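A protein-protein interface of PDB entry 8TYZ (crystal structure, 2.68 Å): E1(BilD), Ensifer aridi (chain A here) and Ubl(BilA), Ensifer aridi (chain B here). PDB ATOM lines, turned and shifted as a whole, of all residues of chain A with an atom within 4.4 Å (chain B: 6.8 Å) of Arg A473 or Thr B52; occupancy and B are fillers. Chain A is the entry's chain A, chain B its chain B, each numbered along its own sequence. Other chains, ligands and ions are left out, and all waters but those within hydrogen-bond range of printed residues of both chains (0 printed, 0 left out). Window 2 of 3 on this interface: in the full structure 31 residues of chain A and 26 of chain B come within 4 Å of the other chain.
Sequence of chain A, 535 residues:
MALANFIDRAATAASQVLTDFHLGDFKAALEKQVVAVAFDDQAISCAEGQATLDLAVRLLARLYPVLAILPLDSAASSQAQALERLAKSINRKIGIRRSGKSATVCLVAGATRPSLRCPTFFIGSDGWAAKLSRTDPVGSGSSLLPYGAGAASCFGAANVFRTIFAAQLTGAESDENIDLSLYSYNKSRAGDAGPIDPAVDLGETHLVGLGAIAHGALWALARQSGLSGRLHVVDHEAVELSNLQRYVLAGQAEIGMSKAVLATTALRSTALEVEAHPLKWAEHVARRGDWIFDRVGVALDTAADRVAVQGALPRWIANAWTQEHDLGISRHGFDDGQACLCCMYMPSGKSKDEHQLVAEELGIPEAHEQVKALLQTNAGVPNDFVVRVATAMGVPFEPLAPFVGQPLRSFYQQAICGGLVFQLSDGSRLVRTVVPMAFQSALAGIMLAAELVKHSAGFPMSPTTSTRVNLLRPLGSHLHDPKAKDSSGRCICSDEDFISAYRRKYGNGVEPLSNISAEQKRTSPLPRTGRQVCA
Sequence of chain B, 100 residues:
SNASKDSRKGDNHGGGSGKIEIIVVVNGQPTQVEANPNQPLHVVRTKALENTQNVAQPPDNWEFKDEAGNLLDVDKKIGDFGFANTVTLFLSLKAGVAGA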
ATOM      1  N   ARG A 162      -1.977 -18.874 -10.801  1.00  0.00           N
ATOM      2  CA  ARG A 162      -3.134 -18.552  -9.970  1.00  0.00           C
ATOM      3  C   ARG A 162      -4.418 -18.424 -10.778  1.00  0.00           C
ATOM      4  O   ARG A 162      -5.508 -18.517 -10.210  1.00  0.00           O
ATOM      5  CB  ARG A 162      -2.890 -17.268  -9.197  1.00  0.00           C
ATOM      6  CG  ARG A 162      -1.627 -17.327  -8.379  1.00  0.00           C
ATOM      7  CD  ARG A 162      -1.655 -16.343  -7.244  1.00  0.00           C
ATOM      8  NE  ARG A 162      -2.039 -15.014  -7.693  1.00  0.00           N
ATOM      9  CZ  ARG A 162      -1.182 -14.037  -7.948  1.00  0.00           C
ATOM     10  NH1 ARG A 162       0.132 -14.221  -7.847  1.00  0.00           N
ATOM     11  NH2 ARG A 162      -1.653 -12.846  -8.301  1.00  0.00           N
ATOM     12  N   THR A 170      -6.789 -19.980  -2.047  1.00  0.00           N
ATOM     13  CA  THR A 170      -7.594 -19.060  -1.249  1.00  0.00           C
ATOM     14  C   THR A 170      -6.915 -17.694  -1.189  1.00  0.00           C
ATOM     15  O   THR A 170      -5.720 -17.599  -0.888  1.00  0.00           O
ATOM     16  CB  THR A 170      -7.858 -19.641   0.149  1.00  0.00           C
ATOM     17  OG1 THR A 170      -9.252 -20.014   0.241  1.00  0.00           O
ATOM     18  CG2 THR A 170      -7.473 -18.656   1.300  1.00  0.00           C
ATOM     19  N   GLY A 171      -7.678 -16.645  -1.503  1.00  0.00           N
ATOM     20  CA  GLY A 171      -7.140 -15.296  -1.521  1.00  0.00           C
ATOM     21  C   GLY A 171      -6.029 -15.072  -2.520  1.00  0.00           C
ATOM     22  O   GLY A 171      -5.136 -14.258  -2.267  1.00  0.00           O
ATOM     23  N   ALA A 172      -6.087 -15.755  -3.662  1.00  0.00           N
ATOM     24  CA  ALA A 172      -5.064 -15.742  -4.707  1.00  0.00           C
ATOM     25  C   ALA A 172      -5.528 -15.016  -5.973  1.00  0.00           C
ATOM     26  O   ALA A 172      -5.372 -15.516  -7.082  1.00  0.00           O
ATOM     27  CB  ALA A 172      -4.648 -17.171  -5.025  1.00  0.00           C
ATOM     28  N   ASN A 470       5.243 -13.016  -1.428  1.00  0.00           N
ATOM     29  CA  ASN A 470       4.371 -14.188  -1.557  1.00  0.00           C
ATOM     30  C   ASN A 470       3.725 -14.194  -2.946  1.00  0.00           C
ATOM     31  O   ASN A 470       2.826 -13.391  -3.226  1.00  0.00           O
ATOM     32  CB  ASN A 470       3.311 -14.196  -0.462  1.00  0.00           C
ATOM     33  CG  ASN A 470       2.266 -15.291  -0.656  1.00  0.00           C
ATOM     34  OD1 ASN A 470       2.345 -16.091  -1.579  1.00  0.00           O
ATOM     35  ND2 ASN A 470       1.273 -15.324   0.227  1.00  0.00           N
ATOM     36  N   LEU A 471       4.153 -15.134  -3.801  1.00  0.00           N
ATOM     37  CA  LEU A 471       3.636 -15.234  -5.163  1.00  0.00           C
ATOM     38  C   LEU A 471       2.358 -16.065  -5.289  1.00  0.00           C
ATOM     39  O   LEU A 471       1.821 -16.168  -6.397  1.00  0.00           O
ATOM     40  CB  LEU A 471       4.702 -15.797  -6.099  1.00  0.00           C
ATOM     41  CG  LEU A 471       5.931 -14.941  -6.400  1.00  0.00           C
ATOM     42  CD1 LEU A 471       7.062 -15.716  -7.197  1.00  0.00           C
ATOM     43  CD2 LEU A 471       5.525 -13.678  -7.117  1.00  0.00           C
ATOM     44  N   LEU A 472       1.850 -16.660  -4.205  1.00  0.00           N
ATOM     45  CA  LEU A 472       0.557 -17.338  -4.234  1.00  0.00           C
ATOM     46  C   LEU A 472      -0.592 -16.408  -3.861  1.00  0.00           C
ATOM     47  O   LEU A 472      -1.675 -16.871  -3.469  1.00  0.00           O
ATOM     48  CB  LEU A 472       0.572 -18.554  -3.330  1.00  0.00           C
ATOM     49  CG  LEU A 472       1.560 -19.582  -3.869  1.00  0.00           C
ATOM     50  CD1 LEU A 472       1.809 -20.674  -2.846  1.00  0.00           C
ATOM     51  CD2 LEU A 472       1.044 -20.141  -5.166  1.00  0.00           C
ATOM     52  N   ARG A 473      -0.367 -15.109  -3.969  1.00  0.00           N
ATOM     53  CA  ARG A 473      -1.335 -14.083  -3.630  1.00  0.00           C
ATOM     54  C   ARG A 473      -0.972 -12.865  -4.454  1.00  0.00           C
ATOM     55  O   ARG A 473       0.088 -12.835  -5.088  1.00  0.00           O
ATOM     56  CB  ARG A 473      -1.313 -13.757  -2.132  1.00  0.00           C
ATOM     57  CG  ARG A 473      -1.890 -14.853  -1.263  1.00  0.00           C
ATOM     58  CD  ARG A 473      -2.405 -14.328   0.035  1.00  0.00           C
ATOM     59  NE  ARG A 473      -3.159 -15.342   0.753  1.00  0.00           N
ATOM     60  CZ  ARG A 473      -3.789 -15.119   1.893  1.00  0.00           C
ATOM     61  NH1 ARG A 473      -3.817 -13.912   2.435  1.00  0.00           N
ATOM     62  NH2 ARG A 473      -4.395 -16.132   2.508  1.00  0.00           N
ATOM     63  N   PRO A 474      -1.827 -11.859  -4.495  1.00  0.00           N
ATOM     64  CA  PRO A 474      -1.414 -10.614  -5.143  1.00  0.00           C
ATOM     65  C   PRO A 474      -0.266 -10.022  -4.353  1.00  0.00           C
ATOM     66  O   PRO A 474      -0.062 -10.357  -3.183  1.00  0.00           O
ATOM     67  CB  PRO A 474      -2.667  -9.743  -5.081  1.00  0.00           C
ATOM     68  CG  PRO A 474      -3.781 -10.755  -4.984  1.00  0.00           C
ATOM     69  CD  PRO A 474      -3.249 -11.818  -4.098  1.00  0.00           C
ATOM     70  N   LEU A 475       0.523  -9.178  -5.017  1.00  0.00           N
ATOM     71  CA  LEU A 475       1.748  -8.669  -4.403  1.00  0.00           C
ATOM     72  C   LEU A 475       1.443  -7.905  -3.110  1.00  0.00           C
ATOM     73  O   LEU A 475       0.472  -7.152  -3.021  1.00  0.00           O
ATOM     74  CB  LEU A 475       2.496  -7.782  -5.401  1.00  0.00           C
ATOM     75  CG  LEU A 475       3.867  -7.248  -5.011  1.00  0.00           C
ATOM     76  CD1 LEU A 475       4.790  -8.395  -4.621  1.00  0.00           C
ATOM     77  CD2 LEU A 475       4.433  -6.448  -6.170  1.00  0.00           C
ATOM     78  N   VAL B  24      -1.636  -4.322  11.065  1.00  0.00           N
ATOM     79  CA  VAL B  24      -0.774  -5.494  11.032  1.00  0.00           C
ATOM     80  C   VAL B  24      -0.435  -5.817   9.574  1.00  0.00           C
ATOM     81  O   VAL B  24      -1.317  -6.148   8.769  1.00  0.00           O
ATOM     82  CB  VAL B  24      -1.437  -6.695  11.722  1.00  0.00           C
ATOM     83  CG1 VAL B  24      -0.421  -7.809  11.924  1.00  0.00           C
ATOM     84  CG2 VAL B  24      -2.050  -6.279  13.026  1.00  0.00           C
ATOM     85  N   VAL B  25       0.840  -5.705   9.218  1.00  0.00           N
ATOM     86  CA  VAL B  25       1.315  -6.232   7.948  1.00  0.00           C
ATOM     87  C   VAL B  25       1.445  -7.740   8.124  1.00  0.00           C
ATOM     88  O   VAL B  25       2.272  -8.208   8.906  1.00  0.00           O
ATOM     89  CB  VAL B  25       2.643  -5.588   7.543  1.00  0.00           C
ATOM     90  CG1 VAL B  25       3.021  -6.009   6.146  1.00  0.00           C
ATOM     91  CG2 VAL B  25       2.518  -4.079   7.610  1.00  0.00           C
ATOM     92  N   VAL B  26       0.595  -8.498   7.438  1.00  0.00           N
ATOM     93  CA  VAL B  26       0.535  -9.949   7.569  1.00  0.00           C
ATOM     94  C   VAL B  26       1.073 -10.543   6.274  1.00  0.00           C
ATOM     95  O   VAL B  26       0.345 -10.626   5.276  1.00  0.00           O
ATOM     96  CB  VAL B  26      -0.885 -10.458   7.851  1.00  0.00           C
ATOM     97  CG1 VAL B  26      -0.900 -11.975   7.994  1.00  0.00           C
ATOM     98  CG2 VAL B  26      -1.478  -9.799   9.069  1.00  0.00           C
ATOM     99  N   ASN B  27       2.346 -10.983   6.295  1.00  0.00           N
ATOM    100  CA  ASN B  27       2.978 -11.628   5.139  1.00  0.00           C
ATOM    101  C   ASN B  27       2.909 -10.684   3.939  1.00  0.00           C
ATOM    102  O   ASN B  27       2.594 -11.082   2.820  1.00  0.00           O
ATOM    103  CB  ASN B  27       2.320 -12.979   4.839  1.00  0.00           C
ATOM    104  CG  ASN B  27       3.149 -13.867   3.937  1.00  0.00           C
ATOM    105  OD1 ASN B  27       4.381 -13.804   3.921  1.00  0.00           O
ATOM    106  ND2 ASN B  27       2.467 -14.736   3.193  1.00  0.00           N
ATOM    107  N   GLN B  29       0.833  -8.241   3.339  1.00  0.00           N
ATOM    108  CA  GLN B  29      -0.501  -7.715   3.132  1.00  0.00           C
ATOM    109  C   GLN B  29      -0.951  -6.960   4.371  1.00  0.00           C
ATOM    110  O   GLN B  29      -1.198  -7.593   5.405  1.00  0.00           O
ATOM    111  CB  GLN B  29      -1.452  -8.860   2.840  1.00  0.00           C
ATOM    112  CG  GLN B  29      -1.398  -9.293   1.431  1.00  0.00           C
ATOM    113  CD  GLN B  29      -2.232 -10.507   1.188  1.00  0.00           C
ATOM    114  OE1 GLN B  29      -2.508 -11.288   2.106  1.00  0.00           O
ATOM    115  NE2 GLN B  29      -2.643 -10.684  -0.057  1.00  0.00           N
ATOM    116  N   PRO B  30      -1.053  -5.637   4.347  1.00  0.00           N
ATOM    117  CA  PRO B  30      -1.508  -4.927   5.548  1.00  0.00           C
ATOM    118  C   PRO B  30      -3.023  -4.979   5.736  1.00  0.00           C
ATOM    119  O   PRO B  30      -3.789  -5.044   4.773  1.00  0.00           O
ATOM    120  CB  PRO B  30      -1.012  -3.489   5.315  1.00  0.00           C
ATOM    121  CG  PRO B  30      -0.731  -3.378   3.881  1.00  0.00           C
ATOM    122  CD  PRO B  30      -0.377  -4.735   3.400  1.00  0.00           C
ATOM    123  N   THR B  31      -3.442  -4.983   7.011  1.00  0.00           N
ATOM    124  CA  THR B  31      -4.840  -4.980   7.441  1.00  0.00           C
ATOM    125  C   THR B  31      -4.932  -4.184   8.734  1.00  0.00           C
ATOM    126  O   THR B  31      -3.917  -3.836   9.342  1.00  0.00           O
ATOM    127  CB  THR B  31      -5.399  -6.409   7.640  1.00  0.00           C
ATOM    128  OG1 THR B  31      -6.834  -6.381   7.735  1.00  0.00           O
ATOM    129  CG2 THR B  31      -4.811  -7.080   8.885  1.00  0.00           C
ATOM    130  N   LYS B  47      -7.397 -11.804  14.859  1.00  0.00           N
ATOM    131  CA  LYS B  47      -8.228 -10.960  14.008  1.00  0.00           C
ATOM    132  C   LYS B  47      -7.524 -10.625  12.703  1.00  0.00           C
ATOM    133  O   LYS B  47      -8.124 -10.710  11.626  1.00  0.00           O
ATOM    134  CB  LYS B  47      -8.628  -9.691  14.755  1.00  0.00           C
ATOM    135  CG  LYS B  47      -9.826  -9.869  15.680  1.00  0.00           C
ATOM    136  CD  LYS B  47      -9.992  -8.652  16.536  1.00  0.00           C
ATOM    137  CE  LYS B  47     -10.925  -8.888  17.676  1.00  0.00           C
ATOM    138  NZ  LYS B  47     -11.038  -7.614  18.423  1.00  0.00           N
ATOM    139  N   ALA B  48      -6.246 -10.248  12.778  1.00  0.00           N
ATOM    140  CA  ALA B  48      -5.507  -9.932  11.562  1.00  0.00           C
ATOM    141  C   ALA B  48      -5.399 -11.146  10.651  1.00  0.00           C
ATOM    142  O   ALA B  48      -5.544 -11.021   9.431  1.00  0.00           O
ATOM    143  CB  ALA B  48      -4.125  -9.385  11.910  1.00  0.00           C
ATOM    144  N   LEU B  49      -5.170 -12.335  11.233  1.00  0.00           N
ATOM    145  CA  LEU B  49      -5.058 -13.581  10.468  1.00  0.00           C
ATOM    146  C   LEU B  49      -6.362 -13.996   9.790  1.00  0.00           C
ATOM    147  O   LEU B  49      -6.328 -14.776   8.831  1.00  0.00           O
ATOM    148  CB  LEU B  49      -4.600 -14.720  11.373  1.00  0.00           C
ATOM    149  CG  LEU B  49      -3.160 -14.747  11.842  1.00  0.00           C
ATOM    150  CD1 LEU B  49      -2.955 -16.003  12.622  1.00  0.00           C
ATOM    151  CD2 LEU B  49      -2.232 -14.694  10.641  1.00  0.00           C
ATOM    152  N   GLU B  50      -7.506 -13.516  10.281  1.00  0.00           N
ATOM    153  CA  GLU B  50      -8.781 -13.742   9.621  1.00  0.00           C
ATOM    154  C   GLU B  50      -9.083 -12.676   8.581  1.00  0.00           C
ATOM    155  O   GLU B  50      -9.665 -12.982   7.530  1.00  0.00           O
ATOM    156  CB  GLU B  50      -9.897 -13.787  10.656  1.00  0.00           C
ATOM    157  CG  GLU B  50     -10.415 -15.173  10.931  1.00  0.00           C
ATOM    158  CD  GLU B  50     -11.260 -15.226  12.174  1.00  0.00           C
ATOM    159  OE1 GLU B  50     -12.207 -14.394  12.298  1.00  0.00           O
ATOM    160  OE2 GLU B  50     -10.938 -16.082  13.041  1.00  0.00           O
ATOM    161  N   ASN B  51      -8.709 -11.425   8.848  1.00  0.00           N
ATOM    162  CA  ASN B  51      -8.923 -10.401   7.840  1.00  0.00           C
ATOM    163  C   ASN B  51      -8.168 -10.739   6.566  1.00  0.00           C
ATOM    164  O   ASN B  51      -8.657 -10.491   5.461  1.00  0.00           O
ATOM    165  CB  ASN B  51      -8.494  -9.033   8.362  1.00  0.00           C
ATOM    166  CG  ASN B  51      -9.337  -8.553   9.520  1.00  0.00           C
ATOM    167  OD1 ASN B  51     -10.511  -8.917   9.664  1.00  0.00           O
ATOM    168  ND2 ASN B  51      -8.733  -7.724  10.361  1.00  0.00           N
ATOM    169  N   THR B  52      -6.988 -11.334   6.703  1.00  0.00           N
ATOM    170  CA  THR B  52      -6.142 -11.687   5.579  1.00  0.00           C
ATOM    171  C   THR B  52      -6.295 -13.146   5.164  1.00  0.00           C
ATOM    172  O   THR B  52      -5.553 -13.602   4.293  1.00  0.00           O
ATOM    173  CB  THR B  52      -4.671 -11.386   5.914  1.00  0.00           C
ATOM    174  OG1 THR B  52      -4.252 -12.173   7.036  1.00  0.00           O
ATOM    175  CG2 THR B  52      -4.463  -9.907   6.235  1.00  0.00           C
ATOM    176  N   GLN B  53      -7.234 -13.885   5.753  1.00  0.00           N
ATOM    177  CA  GLN B  53      -7.493 -15.292   5.433  1.00  0.00           C
ATOM    178  C   GLN B  53      -6.259 -16.177   5.602  1.00  0.00           C
ATOM    179  O   GLN B  53      -6.144 -17.213   4.941  1.00  0.00           O
ATOM    180  CB  GLN B  53      -8.049 -15.455   4.016  1.00  0.00           C
ATOM    181  CG  GLN B  53      -9.060 -14.402   3.605  1.00  0.00           C
ATOM    182  CD  GLN B  53      -9.566 -14.586   2.187  1.00  0.00           C
ATOM    183  OE1 GLN B  53      -9.134 -15.485   1.474  1.00  0.00           O
ATOM    184  NE2 GLN B  53     -10.487 -13.734   1.773  1.00  0.00           N
ATOM    185  N   ASN B  54      -5.327 -15.780   6.467  1.00  0.00           N
ATOM    186  CA  ASN B  54      -4.163 -16.595   6.821  1.00  0.00           C
ATOM    187  C   ASN B  54      -4.479 -17.458   8.046  1.00  0.00           C
ATOM    188  O   ASN B  54      -3.961 -17.255   9.148  1.00  0.00           O
ATOM    189  CB  ASN B  54      -2.950 -15.704   7.080  1.00  0.00           C
ATOM    190  CG  ASN B  54      -2.267 -15.274   5.813  1.00  0.00           C
ATOM    191  OD1 ASN B  54      -1.791 -16.116   5.051  1.00  0.00           O
ATOM    192  ND2 ASN B  54      -2.204 -13.961   5.576  1.00  0.00           N
ATOM    193  N   VAL B  55      -5.370 -18.429   7.857  1.00  0.00           N
ATOM    194  CA  VAL B  55      -5.777 -19.292   8.964  1.00  0.00           C
ATOM    195  C   VAL B  55      -5.374 -20.751   8.766  1.00  0.00           C
ATOM    196  O   VAL B  55      -5.519 -21.542   9.713  1.00  0.00           O
ATOM    197  CB  VAL B  55      -7.295 -19.186   9.265  1.00  0.00           C
ATOM    198  CG1 VAL B  55      -7.668 -17.770   9.745  1.00  0.00           C
ATOM    199  CG2 VAL B  55      -8.165 -19.636   8.087  1.00  0.00           C
ATOM    200  N   TRP B  62       3.457 -17.778  13.166  1.00  0.00           N
ATOM    201  CA  TRP B  62       3.573 -16.365  12.867  1.00  0.00           C
ATOM    202  C   TRP B  62       4.322 -15.675  13.989  1.00  0.00           C
ATOM    203  O   TRP B  62       4.114 -15.976  15.166  1.00  0.00           O
ATOM    204  CB  TRP B  62       2.189 -15.743  12.667  1.00  0.00           C
ATOM    205  CG  TRP B  62       1.468 -16.310  11.472  1.00  0.00           C
ATOM    206  CD1 TRP B  62       0.540 -17.309  11.471  1.00  0.00           C
ATOM    207  CD2 TRP B  62       1.638 -15.918  10.104  1.00  0.00           C
ATOM    208  NE1 TRP B  62       0.126 -17.568  10.188  1.00  0.00           N
ATOM    209  CE2 TRP B  62       0.782 -16.730   9.329  1.00  0.00           C
ATOM    210  CE3 TRP B  62       2.424 -14.952   9.460  1.00  0.00           C
ATOM    211  CZ2 TRP B  62       0.690 -16.612   7.934  1.00  0.00           C
ATOM    212  CZ3 TRP B  62       2.332 -14.834   8.074  1.00  0.00           C
ATOM    213  CH2 TRP B  62       1.468 -15.660   7.328  1.00  0.00           C
ATOM    214  N   LEU B  91       3.253  -9.290  11.126  1.00  0.00           N
ATOM    215  CA  LEU B  91       2.943 -10.703  11.351  1.00  0.00           C
ATOM    216  C   LEU B  91       3.649 -11.487  10.249  1.00  0.00           C
ATOM    217  O   LEU B  91       3.136 -11.616   9.134  1.00  0.00           O
ATOM    218  CB  LEU B  91       1.440 -10.948  11.350  1.00  0.00           C
ATOM    219  CG  LEU B  91       0.834 -11.944  12.329  1.00  0.00           C
ATOM    220  CD1 LEU B  91       1.389 -11.649  13.671  1.00  0.00           C
ATOM    221  CD2 LEU B  91      -0.671 -11.766  12.343  1.00  0.00           C
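Of chain B, only Gln B29 (3.0 Å), Thr B52 (2.6 Å), Gln B53 (3.2 Å) and Asn B54 (3.5 Å) come within 4 Å of Arg A473.
Thr B52 touches just one residue of chain A: Arg A473 (2.6 Å).
Printed residues of chain B within 4 Å of Gly A171: Gln B53 (3.5 Å).
Printed residues of chain A within 4 Å of Gln B29: Arg A473 (3.0 Å).
Of the printed residues of chain B, Asn A470 touches Asn B27 (3.3 Å).
The nearest residue of chain B that does not touch Arg A473 is Asn B27 (5.8 Å).
ND2 of Asn A470 lies close to ND2 of Asn B27 (3.3 Å).
NH1 of Arg A473 sits at hydrogen-bond distance from OE1 of Gln B29.
The backbone carbonyl oxygen (O) of Thr B52 is in hydrogen-bond range of the guanidinium group (NH1) of Arg A473 (2.6 Å).
NH2 of Arg A473 sits at hydrogen-bond distance from O of Gln B53 (3.2 Å).
Gln B53 touches Thr A170.
Gln B53 touches Gly A171 (OE1 to N, 3.5 Å).
NH1 of Arg A473 touches ND2 of Asn B54 (3.5 Å).
NH1 of Arg A162 sits at hydrogen-bond distance from O of Arg A473.
The side-chain amide oxygen of Asn A470 sits at hydrogen-bond distance from the backbone NH of Leu A472.
The backbone NH of Asn B27 sits at hydrogen-bond distance from the backbone carbonyl oxygen of Leu B91 (3.0 Å).
The backbone carbonyl oxygen of Ala B48 lies within hydrogen-bond range of the side-chain hydroxyl of Thr B52 (3.0 Å).
The backbone NH of Asn B54 is in hydrogen-bond range of the backbone carbonyl oxygen of Leu B49 (2.8 Å).
The side-chain hydroxyl of Thr B52 sits at hydrogen-bond distance from the side-chain amide nitrogen of Asn B54 (3.1 Å).
Of the 18 printed residues of chain B, 5 touch a printed residue of chain A.
Among the printed residues, no Asp or Glu carboxylate lies within 4 Å of a Lys or Arg side-chain nitrogen of the other chain.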
